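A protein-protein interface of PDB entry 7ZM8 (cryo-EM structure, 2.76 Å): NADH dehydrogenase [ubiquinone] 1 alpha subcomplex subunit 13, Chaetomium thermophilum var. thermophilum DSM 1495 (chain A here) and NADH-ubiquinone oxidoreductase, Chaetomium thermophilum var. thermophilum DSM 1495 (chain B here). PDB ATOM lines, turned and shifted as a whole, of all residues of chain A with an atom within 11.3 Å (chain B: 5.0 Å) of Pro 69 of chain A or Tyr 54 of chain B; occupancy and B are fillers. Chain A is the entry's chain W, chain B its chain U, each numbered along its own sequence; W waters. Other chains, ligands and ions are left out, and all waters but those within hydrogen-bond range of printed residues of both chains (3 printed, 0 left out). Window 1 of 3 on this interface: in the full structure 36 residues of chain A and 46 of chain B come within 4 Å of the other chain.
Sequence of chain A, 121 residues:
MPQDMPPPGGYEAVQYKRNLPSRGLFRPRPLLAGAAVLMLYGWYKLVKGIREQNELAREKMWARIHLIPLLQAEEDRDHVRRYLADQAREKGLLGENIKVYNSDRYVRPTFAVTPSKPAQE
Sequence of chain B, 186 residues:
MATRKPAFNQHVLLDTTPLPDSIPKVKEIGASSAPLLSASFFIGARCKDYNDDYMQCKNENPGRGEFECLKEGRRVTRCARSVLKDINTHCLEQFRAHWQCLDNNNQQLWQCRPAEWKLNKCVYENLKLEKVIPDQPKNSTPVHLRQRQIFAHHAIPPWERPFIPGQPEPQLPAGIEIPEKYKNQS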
ATOM      1  N   MET A  61      35.165  26.861 -19.095  1.00  0.00           N
ATOM      2  CA  MET A  61      34.494  25.822 -19.904  1.00  0.00           C
ATOM      3  C   MET A  61      33.209  25.406 -19.204  1.00  0.00           C
ATOM      4  O   MET A  61      32.191  25.353 -19.869  1.00  0.00           O
ATOM      5  CB  MET A  61      35.424  24.643 -20.217  1.00  0.00           C
ATOM      6  CG  MET A  61      36.527  24.986 -21.206  1.00  0.00           C
ATOM      7  SD  MET A  61      35.950  25.424 -22.874  1.00  0.00           S
ATOM      8  CE  MET A  61      36.223  27.195 -22.886  1.00  0.00           C
ATOM      9  N   TRP A  62      33.275  25.128 -17.905  1.00  0.00           N
ATOM     10  CA  TRP A  62      32.102  24.699 -17.108  1.00  0.00           C
ATOM     11  C   TRP A  62      31.041  25.788 -17.114  1.00  0.00           C
ATOM     12  O   TRP A  62      29.866  25.438 -17.099  1.00  0.00           O
ATOM     13  CB  TRP A  62      32.567  24.287 -15.711  1.00  0.00           C
ATOM     14  CG  TRP A  62      33.150  22.909 -15.724  1.00  0.00           C
ATOM     15  CD1 TRP A  62      34.458  22.559 -15.566  1.00  0.00           C
ATOM     16  CD2 TRP A  62      32.438  21.687 -15.975  1.00  0.00           C
ATOM     17  NE1 TRP A  62      34.605  21.204 -15.671  1.00  0.00           N
ATOM     18  CE2 TRP A  62      33.383  20.643 -15.926  1.00  0.00           C
ATOM     19  CE3 TRP A  62      31.097  21.374 -16.212  1.00  0.00           C
ATOM     20  CZ2 TRP A  62      33.027  19.311 -16.114  1.00  0.00           C
ATOM     21  CZ3 TRP A  62      30.746  20.058 -16.397  1.00  0.00           C
ATOM     22  CH2 TRP A  62      31.698  19.043 -16.348  1.00  0.00           C
ATOM     23  N   ALA A  63      31.451  27.045 -17.196  1.00  0.00           N
ATOM     24  CA  ALA A  63      30.521  28.187 -17.252  1.00  0.00           C
ATOM     25  C   ALA A  63      29.755  28.178 -18.582  1.00  0.00           C
ATOM     26  O   ALA A  63      28.542  28.396 -18.536  1.00  0.00           O
ATOM     27  CB  ALA A  63      31.333  29.437 -17.090  1.00  0.00           C
ATOM     28  N   ARG A  64      30.426  27.906 -19.704  1.00  0.00           N
ATOM     29  CA  ARG A  64      29.796  27.802 -21.042  1.00  0.00           C
ATOM     30  C   ARG A  64      29.016  26.492 -21.178  1.00  0.00           C
ATOM     31  O   ARG A  64      27.998  26.526 -21.857  1.00  0.00           O
ATOM     32  CB  ARG A  64      30.834  28.003 -22.147  1.00  0.00           C
ATOM     33  CG  ARG A  64      31.517  29.356 -22.180  1.00  0.00           C
ATOM     34  CD  ARG A  64      32.463  29.243 -23.351  1.00  0.00           C
ATOM     35  NE  ARG A  64      33.159  30.483 -23.614  1.00  0.00           N
ATOM     36  CZ  ARG A  64      34.002  30.664 -24.609  1.00  0.00           C
ATOM     37  NH1 ARG A  64      34.576  31.837 -24.780  1.00  0.00           N
ATOM     38  NH2 ARG A  64      34.252  29.679 -25.446  1.00  0.00           N
ATOM     39  N   ILE A  65      29.424  25.404 -20.522  1.00  0.00           N
ATOM     40  CA  ILE A  65      28.655  24.126 -20.531  1.00  0.00           C
ATOM     41  C   ILE A  65      27.282  24.296 -19.869  1.00  0.00           C
ATOM     42  O   ILE A  65      26.299  23.818 -20.445  1.00  0.00           O
ATOM     43  CB  ILE A  65      29.475  22.982 -19.910  1.00  0.00           C
ATOM     44  CG1 ILE A  65      30.560  22.475 -20.861  1.00  0.00           C
ATOM     45  CG2 ILE A  65      28.579  21.859 -19.406  1.00  0.00           C
ATOM     46  CD1 ILE A  65      31.746  21.873 -20.153  1.00  0.00           C
ATOM     47  N   HIS A  66      27.188  24.975 -18.732  1.00  0.00           N
ATOM     48  CA  HIS A  66      25.899  25.126 -18.014  1.00  0.00           C
ATOM     49  C   HIS A  66      24.949  26.002 -18.822  1.00  0.00           C
ATOM     50  O   HIS A  66      23.746  25.918 -18.591  1.00  0.00           O
ATOM     51  CB  HIS A  66      26.073  25.629 -16.587  1.00  0.00           C
ATOM     52  CG  HIS A  66      26.891  24.764 -15.690  1.00  0.00           C
ATOM     53  ND1 HIS A  66      26.888  23.391 -15.777  1.00  0.00           N
ATOM     54  CD2 HIS A  66      27.705  25.072 -14.662  1.00  0.00           C
ATOM     55  CE1 HIS A  66      27.679  22.890 -14.858  1.00  0.00           C
ATOM     56  NE2 HIS A  66      28.192  23.899 -14.164  1.00  0.00           N
ATOM     57  N   LEU A  67      25.479  26.770 -19.777  1.00  0.00           N
ATOM     58  CA  LEU A  67      24.648  27.680 -20.606  1.00  0.00           C
ATOM     59  C   LEU A  67      24.361  27.057 -21.972  1.00  0.00           C
ATOM     60  O   LEU A  67      23.429  27.520 -22.621  1.00  0.00           O
ATOM     61  CB  LEU A  67      25.407  28.999 -20.776  1.00  0.00           C
ATOM     62  CG  LEU A  67      25.500  29.894 -19.545  1.00  0.00           C
ATOM     63  CD1 LEU A  67      26.300  31.147 -19.860  1.00  0.00           C
ATOM     64  CD2 LEU A  67      24.116  30.261 -19.036  1.00  0.00           C
ATOM     65  N   ILE A  68      25.123  26.045 -22.386  1.00  0.00           N
ATOM     66  CA  ILE A  68      24.979  25.474 -23.762  1.00  0.00           C
ATOM     67  C   ILE A  68      23.571  24.904 -23.984  1.00  0.00           C
ATOM     68  O   ILE A  68      23.017  25.197 -25.049  1.00  0.00           O
ATOM     69  CB  ILE A  68      26.092  24.447 -24.073  1.00  0.00           C
ATOM     70  CG1 ILE A  68      27.350  25.110 -24.634  1.00  0.00           C
ATOM     71  CG2 ILE A  68      25.597  23.350 -25.003  1.00  0.00           C
ATOM     72  CD1 ILE A  68      28.513  24.165 -24.797  1.00  0.00           C
ATOM     73  N   PRO A  69      22.942  24.137 -23.064  1.00  0.00           N
ATOM     74  CA  PRO A  69      21.598  23.620 -23.311  1.00  0.00           C
ATOM     75  C   PRO A  69      20.494  24.676 -23.467  1.00  0.00           C
ATOM     76  O   PRO A  69      19.684  24.482 -24.331  1.00  0.00           O
ATOM     77  CB  PRO A  69      21.354  22.667 -22.133  1.00  0.00           C
ATOM     78  CG  PRO A  69      22.740  22.288 -21.695  1.00  0.00           C
ATOM     79  CD  PRO A  69      23.493  23.590 -21.819  1.00  0.00           C
ATOM     80  N   LEU A  70      20.491  25.743 -22.661  1.00  0.00           N
ATOM     81  CA  LEU A  70      19.483  26.825 -22.848  1.00  0.00           C
ATOM     82  C   LEU A  70      19.721  27.519 -24.180  1.00  0.00           C
ATOM     83  O   LEU A  70      18.752  27.876 -24.845  1.00  0.00           O
ATOM     84  CB  LEU A  70      19.425  27.811 -21.677  1.00  0.00           C
ATOM     85  CG  LEU A  70      20.642  28.684 -21.385  1.00  0.00           C
ATOM     86  CD1 LEU A  70      20.475  30.072 -21.987  1.00  0.00           C
ATOM     87  CD2 LEU A  70      20.828  28.810 -19.883  1.00  0.00           C
ATOM     88  N   LEU A  71      20.973  27.692 -24.548  1.00  0.00           N
ATOM     89  CA  LEU A  71      21.249  28.452 -25.779  1.00  0.00           C
ATOM     90  C   LEU A  71      20.920  27.594 -26.995  1.00  0.00           C
ATOM     91  O   LEU A  71      20.401  28.155 -27.955  1.00  0.00           O
ATOM     92  CB  LEU A  71      22.676  29.014 -25.761  1.00  0.00           C
ATOM     93  CG  LEU A  71      22.882  30.266 -24.919  1.00  0.00           C
ATOM     94  CD1 LEU A  71      24.359  30.516 -24.673  1.00  0.00           C
ATOM     95  CD2 LEU A  71      22.225  31.464 -25.572  1.00  0.00           C
ATOM     96  N   GLN A  72      21.218  26.301 -26.945  1.00  0.00           N
ATOM     97  CA  GLN A  72      20.922  25.400 -28.049  1.00  0.00           C
ATOM     98  C   GLN A  72      19.426  25.149 -28.183  1.00  0.00           C
ATOM     99  O   GLN A  72      18.938  24.918 -29.292  1.00  0.00           O
ATOM    100  CB  GLN A  72      21.668  24.083 -27.853  1.00  0.00           C
ATOM    101  CG  GLN A  72      21.700  23.195 -29.074  1.00  0.00           C
ATOM    102  CD  GLN A  72      22.308  23.875 -30.274  1.00  0.00           C
ATOM    103  OE1 GLN A  72      23.434  24.356 -30.223  1.00  0.00           O
ATOM    104  NE2 GLN A  72      21.563  23.918 -31.368  1.00  0.00           N
ATOM    105  N   ALA A  73      18.692  25.180 -27.073  1.00  0.00           N
ATOM    106  CA  ALA A  73      17.253  24.948 -27.123  1.00  0.00           C
ATOM    107  C   ALA A  73      16.540  26.070 -27.860  1.00  0.00           C
ATOM    108  O   ALA A  73      15.620  25.821 -28.645  1.00  0.00           O
ATOM    109  CB  ALA A  73      16.706  24.793 -25.708  1.00  0.00           C
ATOM    110  N   GLU A  74      16.955  27.316 -27.621  1.00  0.00           N
ATOM    111  CA  GLU A  74      16.354  28.451 -28.306  1.00  0.00           C
ATOM    112  C   GLU A  74      16.731  28.456 -29.781  1.00  0.00           C
ATOM    113  O   GLU A  74      15.940  28.880 -30.630  1.00  0.00           O
ATOM    114  CB  GLU A  74      16.785  29.742 -27.603  1.00  0.00           C
ATOM    115  CG  GLU A  74      16.088  31.034 -28.019  1.00  0.00           C
ATOM    116  CD  GLU A  74      16.694  31.678 -29.248  1.00  0.00           C
ATOM    117  OE1 GLU A  74      17.906  31.497 -29.477  1.00  0.00           O
ATOM    118  OE2 GLU A  74      15.965  32.368 -29.992  1.00  0.00           O
ATOM    119  N   GLU A  75      17.929  27.972 -30.103  1.00  0.00           N
ATOM    120  CA  GLU A  75      18.316  27.792 -31.495  1.00  0.00           C
ATOM    121  C   GLU A  75      17.499  26.690 -32.162  1.00  0.00           C
ATOM    122  O   GLU A  75      17.127  26.809 -33.334  1.00  0.00           O
ATOM    123  CB  GLU A  75      19.808  27.484 -31.577  1.00  0.00           C
ATOM    124  CG  GLU A  75      20.436  27.666 -32.958  1.00  0.00           C
ATOM    125  CD  GLU A  75      20.563  29.123 -33.381  1.00  0.00           C
ATOM    126  OE1 GLU A  75      20.593  30.011 -32.500  1.00  0.00           O
ATOM    127  OE2 GLU A  75      20.641  29.378 -34.602  1.00  0.00           O
ATOM    128  N   ASP A  76      17.202  25.616 -31.426  1.00  0.00           N
ATOM    129  CA  ASP A  76      16.506  24.472 -32.007  1.00  0.00           C
ATOM    130  C   ASP A  76      15.065  24.804 -32.361  1.00  0.00           C
ATOM    131  O   ASP A  76      14.538  24.304 -33.360  1.00  0.00           O
ATOM    132  CB  ASP A  76      16.552  23.287 -31.050  1.00  0.00           C
ATOM    133  CG  ASP A  76      17.898  22.628 -31.024  1.00  0.00           C
ATOM    134  OD1 ASP A  76      18.732  22.972 -31.881  1.00  0.00           O
ATOM    135  OD2 ASP A  76      18.126  21.765 -30.151  1.00  0.00           O
ATOM    136  N   ARG A  77      14.400  25.619 -31.546  1.00  0.00           N
ATOM    137  CA  ARG A  77      13.049  26.038 -31.893  1.00  0.00           C
ATOM    138  C   ARG A  77      13.060  26.929 -33.123  1.00  0.00           C
ATOM    139  O   ARG A  77      12.132  26.889 -33.935  1.00  0.00           O
ATOM    140  CB  ARG A  77      12.399  26.751 -30.715  1.00  0.00           C
ATOM    141  CG  ARG A  77      12.159  25.857 -29.533  1.00  0.00           C
ATOM    142  CD  ARG A  77      11.530  26.603 -28.387  1.00  0.00           C
ATOM    143  NE  ARG A  77      12.482  27.448 -27.679  1.00  0.00           N
ATOM    144  CZ  ARG A  77      13.051  27.128 -26.523  1.00  0.00           C
ATOM    145  NH1 ARG A  77      12.780  25.975 -25.935  1.00  0.00           N
ATOM    146  NH2 ARG A  77      13.899  27.968 -25.954  1.00  0.00           N
ATOM    147  N   ASP A  78      14.107  27.737 -33.275  1.00  0.00           N
ATOM    148  CA  ASP A  78      14.225  28.593 -34.445  1.00  0.00           C
ATOM    149  C   ASP A  78      14.450  27.770 -35.706  1.00  0.00           C
ATOM    150  O   ASP A  78      13.906  28.088 -36.766  1.00  0.00           O
ATOM    151  CB  ASP A  78      15.362  29.587 -34.239  1.00  0.00           C
ATOM    152  CG  ASP A  78      15.196  30.839 -35.059  1.00  0.00           C
ATOM    153  OD1 ASP A  78      14.210  31.565 -34.829  1.00  0.00           O
ATOM    154  OD2 ASP A  78      16.056  31.106 -35.922  1.00  0.00           O
ATOM    155  N   HIS A  79      15.230  26.704 -35.612  1.00  0.00           N
ATOM    156  CA  HIS A  79      15.466  25.808 -36.767  1.00  0.00           C
ATOM    157  C   HIS A  79      14.191  25.039 -37.079  1.00  0.00           C
ATOM    158  O   HIS A  79      13.913  24.838 -38.260  1.00  0.00           O
ATOM    159  CB  HIS A  79      16.657  24.891 -36.504  1.00  0.00           C
ATOM    160  CG  HIS A  79      17.963  25.584 -36.640  1.00  0.00           C
ATOM    161  ND1 HIS A  79      18.837  25.304 -37.657  1.00  0.00           N
ATOM    162  CD2 HIS A  79      18.531  26.564 -35.909  1.00  0.00           C
ATOM    163  CE1 HIS A  79      19.897  26.062 -37.530  1.00  0.00           C
ATOM    164  NE2 HIS A  79      19.733  26.847 -36.477  1.00  0.00           N
ATOM    165  N   VAL A  80      13.455  24.610 -36.057  1.00  0.00           N
ATOM    166  CA  VAL A  80      12.149  23.939 -36.313  1.00  0.00           C
ATOM    167  C   VAL A  80      11.217  24.963 -36.974  1.00  0.00           C
ATOM    168  O   VAL A  80      10.599  24.605 -37.982  1.00  0.00           O
ATOM    169  CB  VAL A  80      11.563  23.322 -35.024  1.00  0.00           C
ATOM    170  CG1 VAL A  80      10.122  22.879 -35.197  1.00  0.00           C
ATOM    171  CG2 VAL A  80      12.413  22.168 -34.519  1.00  0.00           C
ATOM    172  N   TYR A 106      17.441  15.908 -40.186  1.00  0.00           N
ATOM    173  CA  TYR A 106      17.344  17.366 -40.431  1.00  0.00           C
ATOM    174  C   TYR A 106      18.721  17.841 -40.852  1.00  0.00           C
ATOM    175  O   TYR A 106      19.676  17.728 -40.083  1.00  0.00           O
ATOM    176  CB  TYR A 106      16.874  18.161 -39.212  1.00  0.00           C
ATOM    177  CG  TYR A 106      17.073  19.647 -39.353  1.00  0.00           C
ATOM    178  CD1 TYR A 106      16.396  20.369 -40.320  1.00  0.00           C
ATOM    179  CD2 TYR A 106      17.960  20.328 -38.537  1.00  0.00           C
ATOM    180  CE1 TYR A 106      16.589  21.729 -40.472  1.00  0.00           C
ATOM    181  CE2 TYR A 106      18.166  21.687 -38.675  1.00  0.00           C
ATOM    182  CZ  TYR A 106      17.475  22.389 -39.643  1.00  0.00           C
ATOM    183  OH  TYR A 106      17.675  23.730 -39.779  1.00  0.00           O
ATOM    184  N   ARG A 108      20.825  21.183 -41.875  1.00  0.00           N
ATOM    185  CA  ARG A 108      20.728  22.659 -41.725  1.00  0.00           C
ATOM    186  C   ARG A 108      20.840  23.312 -43.101  1.00  0.00           C
ATOM    187  O   ARG A 108      21.813  22.980 -43.797  1.00  0.00           O
ATOM    188  CB  ARG A 108      21.733  23.186 -40.697  1.00  0.00           C
ATOM    189  CG  ARG A 108      21.492  22.719 -39.271  1.00  0.00           C
ATOM    190  CD  ARG A 108      22.753  22.856 -38.445  1.00  0.00           C
ATOM    191  NE  ARG A 108      23.079  24.236 -38.138  1.00  0.00           N
ATOM    192  CZ  ARG A 108      22.805  24.836 -36.988  1.00  0.00           C
ATOM    193  NH1 ARG A 108      23.140  26.102 -36.807  1.00  0.00           N
ATOM    194  NH2 ARG A 108      22.190  24.170 -36.027  1.00  0.00           N
ATOM    195  N   TYR B  50      18.323  18.520 -15.896  1.00  0.00           N
ATOM    196  CA  TYR B  50      17.490  18.812 -17.083  1.00  0.00           C
ATOM    197  C   TYR B  50      18.404  19.143 -18.247  1.00  0.00           C
ATOM    198  O   TYR B  50      18.080  18.739 -19.355  1.00  0.00           O
ATOM    199  CB  TYR B  50      16.548  19.965 -16.744  1.00  0.00           C
ATOM    200  CG  TYR B  50      15.611  19.661 -15.607  1.00  0.00           C
ATOM    201  CD1 TYR B  50      14.440  18.961 -15.823  1.00  0.00           C
ATOM    202  CD2 TYR B  50      15.901  20.055 -14.313  1.00  0.00           C
ATOM    203  CE1 TYR B  50      13.569  18.669 -14.790  1.00  0.00           C
ATOM    204  CE2 TYR B  50      15.046  19.763 -13.267  1.00  0.00           C
ATOM    205  CZ  TYR B  50      13.876  19.068 -13.505  1.00  0.00           C
ATOM    206  OH  TYR B  50      13.021  18.782 -12.483  1.00  0.00           O
ATOM    207  N   ASN B  51      19.511  19.838 -17.989  1.00  0.00           N
ATOM    208  CA  ASN B  51      20.509  20.216 -19.026  1.00  0.00           C
ATOM    209  C   ASN B  51      21.128  18.938 -19.565  1.00  0.00           C
ATOM    210  O   ASN B  51      21.434  18.895 -20.743  1.00  0.00           O
ATOM    211  CB  ASN B  51      21.525  21.247 -18.522  1.00  0.00           C
ATOM    212  CG  ASN B  51      20.931  22.544 -18.041  1.00  0.00           C
ATOM    213  OD1 ASN B  51      19.732  22.761 -18.160  1.00  0.00           O
ATOM    214  ND2 ASN B  51      21.769  23.405 -17.488  1.00  0.00           N
ATOM    215  N   ASP B  52      21.259  17.932 -18.719  1.00  0.00           N
ATOM    216  CA  ASP B  52      21.922  16.671 -19.121  1.00  0.00           C
ATOM    217  C   ASP B  52      20.910  15.795 -19.836  1.00  0.00           C
ATOM    218  O   ASP B  52      21.289  15.197 -20.830  1.00  0.00           O
ATOM    219  CB  ASP B  52      22.548  15.996 -17.906  1.00  0.00           C
ATOM    220  CG  ASP B  52      23.855  16.618 -17.455  1.00  0.00           C
ATOM    221  OD1 ASP B  52      24.544  17.213 -18.299  1.00  0.00           O
ATOM    222  OD2 ASP B  52      24.172  16.493 -16.260  1.00  0.00           O
ATOM    223  N   ASP B  53      19.653  15.819 -19.404  1.00  0.00           N
ATOM    224  CA  ASP B  53      18.605  15.039 -20.097  1.00  0.00           C
ATOM    225  C   ASP B  53      18.507  15.538 -21.533  1.00  0.00           C
ATOM    226  O   ASP B  53      18.411  14.702 -22.438  1.00  0.00           O
ATOM    227  CB  ASP B  53      17.264  15.163 -19.384  1.00  0.00           C
ATOM    228  CG  ASP B  53      16.233  14.157 -19.853  1.00  0.00           C
ATOM    229  OD1 ASP B  53      16.617  13.001 -20.099  1.00  0.00           O
ATOM    230  OD2 ASP B  53      15.062  14.545 -19.970  1.00  0.00           O
ATOM    231  N   TYR B  54      18.535  16.844 -21.737  1.00  0.00           N
ATOM    232  CA  TYR B  54      18.336  17.392 -23.095  1.00  0.00           C
ATOM    233  C   TYR B  54      19.453  16.941 -24.025  1.00  0.00           C
ATOM    234  O   TYR B  54      19.165  16.528 -25.149  1.00  0.00           O
ATOM    235  CB  TYR B  54      18.184  18.903 -22.989  1.00  0.00           C
ATOM    236  CG  TYR B  54      18.222  19.662 -24.283  1.00  0.00           C
ATOM    237  CD1 TYR B  54      17.141  19.657 -25.144  1.00  0.00           C
ATOM    238  CD2 TYR B  54      19.338  20.400 -24.625  1.00  0.00           C
ATOM    239  CE1 TYR B  54      17.173  20.368 -26.327  1.00  0.00           C
ATOM    240  CE2 TYR B  54      19.390  21.115 -25.805  1.00  0.00           C
ATOM    241  CZ  TYR B  54      18.303  21.095 -26.651  1.00  0.00           C
ATOM    242  OH  TYR B  54      18.360  21.807 -27.803  1.00  0.00           O
ATOM    243  N   MET B  55      20.686  17.032 -23.561  1.00  0.00           N
ATOM    244  CA  MET B  55      21.851  16.629 -24.384  1.00  0.00           C
ATOM    245  C   MET B  55      21.821  15.127 -24.627  1.00  0.00           C
ATOM    246  O   MET B  55      22.067  14.725 -25.758  1.00  0.00           O
ATOM    247  CB  MET B  55      23.134  17.075 -23.683  1.00  0.00           C
ATOM    248  CG  MET B  55      23.183  18.575 -23.481  1.00  0.00           C
ATOM    249  SD  MET B  55      23.149  19.508 -25.027  1.00  0.00           S
ATOM    250  CE  MET B  55      24.770  19.116 -25.681  1.00  0.00           C
ATOM    251  N   GLN B  56      21.481  14.343 -23.605  1.00  0.00           N
ATOM    252  CA  GLN B  56      21.383  12.871 -23.720  1.00  0.00           C
ATOM    253  C   GLN B  56      20.285  12.491 -24.715  1.00  0.00           C
ATOM    254  O   GLN B  56      20.528  11.596 -25.508  1.00  0.00           O
ATOM    255  CB  GLN B  56      21.146  12.274 -22.338  1.00  0.00           C
ATOM    256  CG  GLN B  56      22.346  11.556 -21.753  1.00  0.00           C
ATOM    257  CD  GLN B  56      21.988  11.046 -20.382  1.00  0.00           C
ATOM    258  OE1 GLN B  56      21.076  11.554 -19.737  1.00  0.00           O
ATOM    259  NE2 GLN B  56      22.705  10.032 -19.927  1.00  0.00           N
ATOM    260  N   CYS B  57      19.134  13.172 -24.691  1.00  0.00           N
ATOM    261  CA  CYS B  57      17.989  12.969 -25.631  1.00  0.00           C
ATOM    262  C   CYS B  57      18.392  13.189 -27.065  1.00  0.00           C
ATOM    263  O   CYS B  57      17.961  12.408 -27.904  1.00  0.00           O
ATOM    264  CB  CYS B  57      16.925  14.038 -25.412  1.00  0.00           C
ATOM    265  SG  CYS B  57      15.457  13.963 -26.482  1.00  0.00           S
ATOM    266  N   LYS B  58      19.014  14.327 -27.361  1.00  0.00           N
ATOM    267  CA  LYS B  58      19.413  14.660 -28.753  1.00  0.00           C
ATOM    268  C   LYS B  58      20.418  13.634 -29.241  1.00  0.00           C
ATOM    269  O   LYS B  58      20.463  13.400 -30.443  1.00  0.00           O
ATOM    270  CB  LYS B  58      20.094  16.027 -28.771  1.00  0.00           C
ATOM    271  CG  LYS B  58      19.202  17.220 -28.466  1.00  0.00           C
ATOM    272  CD  LYS B  58      19.694  18.481 -29.124  1.00  0.00           C
ATOM    273  CE  LYS B  58      19.827  18.336 -30.624  1.00  0.00           C
ATOM    274  NZ  LYS B  58      19.892  19.654 -31.300  1.00  0.00           N
ATOM    275  N   CYS B  69      13.229  16.424 -29.632  1.00  0.00           N
ATOM    276  CA  CYS B  69      13.753  16.779 -28.279  1.00  0.00           C
ATOM    277  C   CYS B  69      13.215  18.158 -27.873  1.00  0.00           C
ATOM    278  O   CYS B  69      13.844  18.800 -27.035  1.00  0.00           O
ATOM    279  CB  CYS B  69      15.268  16.629 -28.152  1.00  0.00           C
ATOM    280  SG  CYS B  69      15.855  14.916 -28.264  1.00  0.00           S
ATOM    281  N   GLU B  72      11.997  18.626 -23.929  1.00  0.00           N
ATOM    282  CA  GLU B  72      13.178  18.729 -23.045  1.00  0.00           C
ATOM    283  C   GLU B  72      13.800  20.120 -23.132  1.00  0.00           C
ATOM    284  O   GLU B  72      14.238  20.614 -22.097  1.00  0.00           O
ATOM    285  CB  GLU B  72      14.152  17.605 -23.387  1.00  0.00           C
ATOM    286  CG  GLU B  72      13.625  16.217 -23.076  1.00  0.00           C
ATOM    287  CD  GLU B  72      12.603  15.665 -24.054  1.00  0.00           C
ATOM    288  OE1 GLU B  72      12.590  16.117 -25.211  1.00  0.00           O
ATOM    289  OE2 GLU B  72      11.813  14.793 -23.648  1.00  0.00           O
ATOM    290  N   GLY B  73      13.873  20.714 -24.316  1.00  0.00           N
ATOM    291  CA  GLY B  73      14.399  22.085 -24.446  1.00  0.00           C
ATOM    292  C   GLY B  73      13.524  23.051 -23.706  1.00  0.00           C
ATOM    293  O   GLY B  73      14.054  23.995 -23.136  1.00  0.00           O
ATOM    294  N   VAL B  76      14.404  22.831 -20.025  1.00  0.00           N
ATOM    295  CA  VAL B  76      15.661  23.554 -19.689  1.00  0.00           C
ATOM    296  C   VAL B  76      15.433  25.069 -19.634  1.00  0.00           C
ATOM    297  O   VAL B  76      16.010  25.698 -18.755  1.00  0.00           O
ATOM    298  CB  VAL B  76      16.859  23.156 -20.576  1.00  0.00           C
ATOM    299  CG1 VAL B  76      17.098  21.664 -20.627  1.00  0.00           C
ATOM    300  CG2 VAL B  76      16.833  23.756 -21.967  1.00  0.00           C
HETATM  301  O   HOH W   1      21.477  25.570 -19.786  1.00  0.00           O
HETATM  302  O   HOH W   2      16.118  19.575 -29.495  1.00  0.00           O
HETATM  303  O   HOH W   3      24.789  21.701 -17.236  1.00  0.00           O
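OD2 of Asp 76 of chain A lies close to OH of Tyr 54 of chain B, at 2.4 Å.
The backbone NH of Ala 73 of chain A sits close to the side-chain hydroxyl of Tyr 54 of chain B.
NZ of Lys 58 of chain B lies within salt-bridge range of OD2 of Asp 76 of chain A (3.0 Å).
O of His 66 of chain A sits at hydrogen-bond distance from ND2 of Asn 51 of chain B (3.4 Å).
The side-chain hydroxyl (OH) of Tyr 54 of chain B sits at hydrogen-bond distance from the backbone carbonyl oxygen (O) of Gln 72 of chain A (3.5 Å).
Printed residues of chain B within 4 Å of His 66 of chain A: Asn 51 (3.4 Å).
Of the printed residues of chain B, Ala 73 of chain A touches Tyr 54 (3.4 Å), Gly 73 (3.8 Å) and Val 76 (3.9 Å).
Printed residues of chain B within 4 Å of Asp 76 of chain A: Tyr 54 (2.4 Å) and Lys 58 (3.0 Å).
Of chain A, only His 66 and Pro 69 come within 4 Å of Asn 51 of chain B.
Of chain A, only Pro 69, Gln 72, Ala 73 and Asp 76 come within 4 Å of Tyr 54 of chain B.
No residue of chain A comes within 4 Å of Cys 57 of chain B.
Lys 58 of chain B touches just one residue of chain A: Asp 76 (3.0 Å).
Cys 69 of chain B touches none of the printed residues of chain A.
Gly 73 of chain B touches two residues of chain A.
Hydrophobic or aromatic side chains of chain B within 4 Å of the printed part of chain A: Tyr 54 and Val 76.
Along chain B the printed residues that touch a printed residue of chain A span positions 51 to 76.
The side-chain amide nitrogen of Gln 72 of chain A is in hydrogen-bond range of the side-chain carboxylate of Asp 76 of chain A (3.0 Å).
The backbone NH (N) of Lys 58 of chain B lies within hydrogen-bond range of the side-chain sulfur (SG) of Cys 69 of chain B (3.3 Å).
SG of Cys 69 of chain B is disulfide-bonded to SG of Cys 57 of chain B (2.1 Å).
Water W1 lies within hydrogen-bond range of O of His 66 of chain A, N of Leu 70 of chain A and ND2 of Asn 51 of chain B.
Water W2 lies within hydrogen-bond range of OD2 of Asp 76 of chain A (3.0 Å) and O of Cys 69 of chain B (3.4 Å).
Water W3 lies within hydrogen-bond range of ND1 of His 66 of chain A (3.1 Å) and ND2 of Asn 51 of chain B (3.5 Å).
Asn 51 of chain B touches Pro 69 of chain A.
Tyr 54 of chain B touches Pro 69 of chain A.
Val 76 of chain B touches Pro 69 of chain A.
Gly 73 of chain B touches Ala 73 of chain A (CA to CB, 3.8 Å).
CB of Ala 73 of chain A touches CG2 of Val 76 of chain B, at 3.9 Å.
Arg 77 of chain A touches Gly 73 of chain B.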
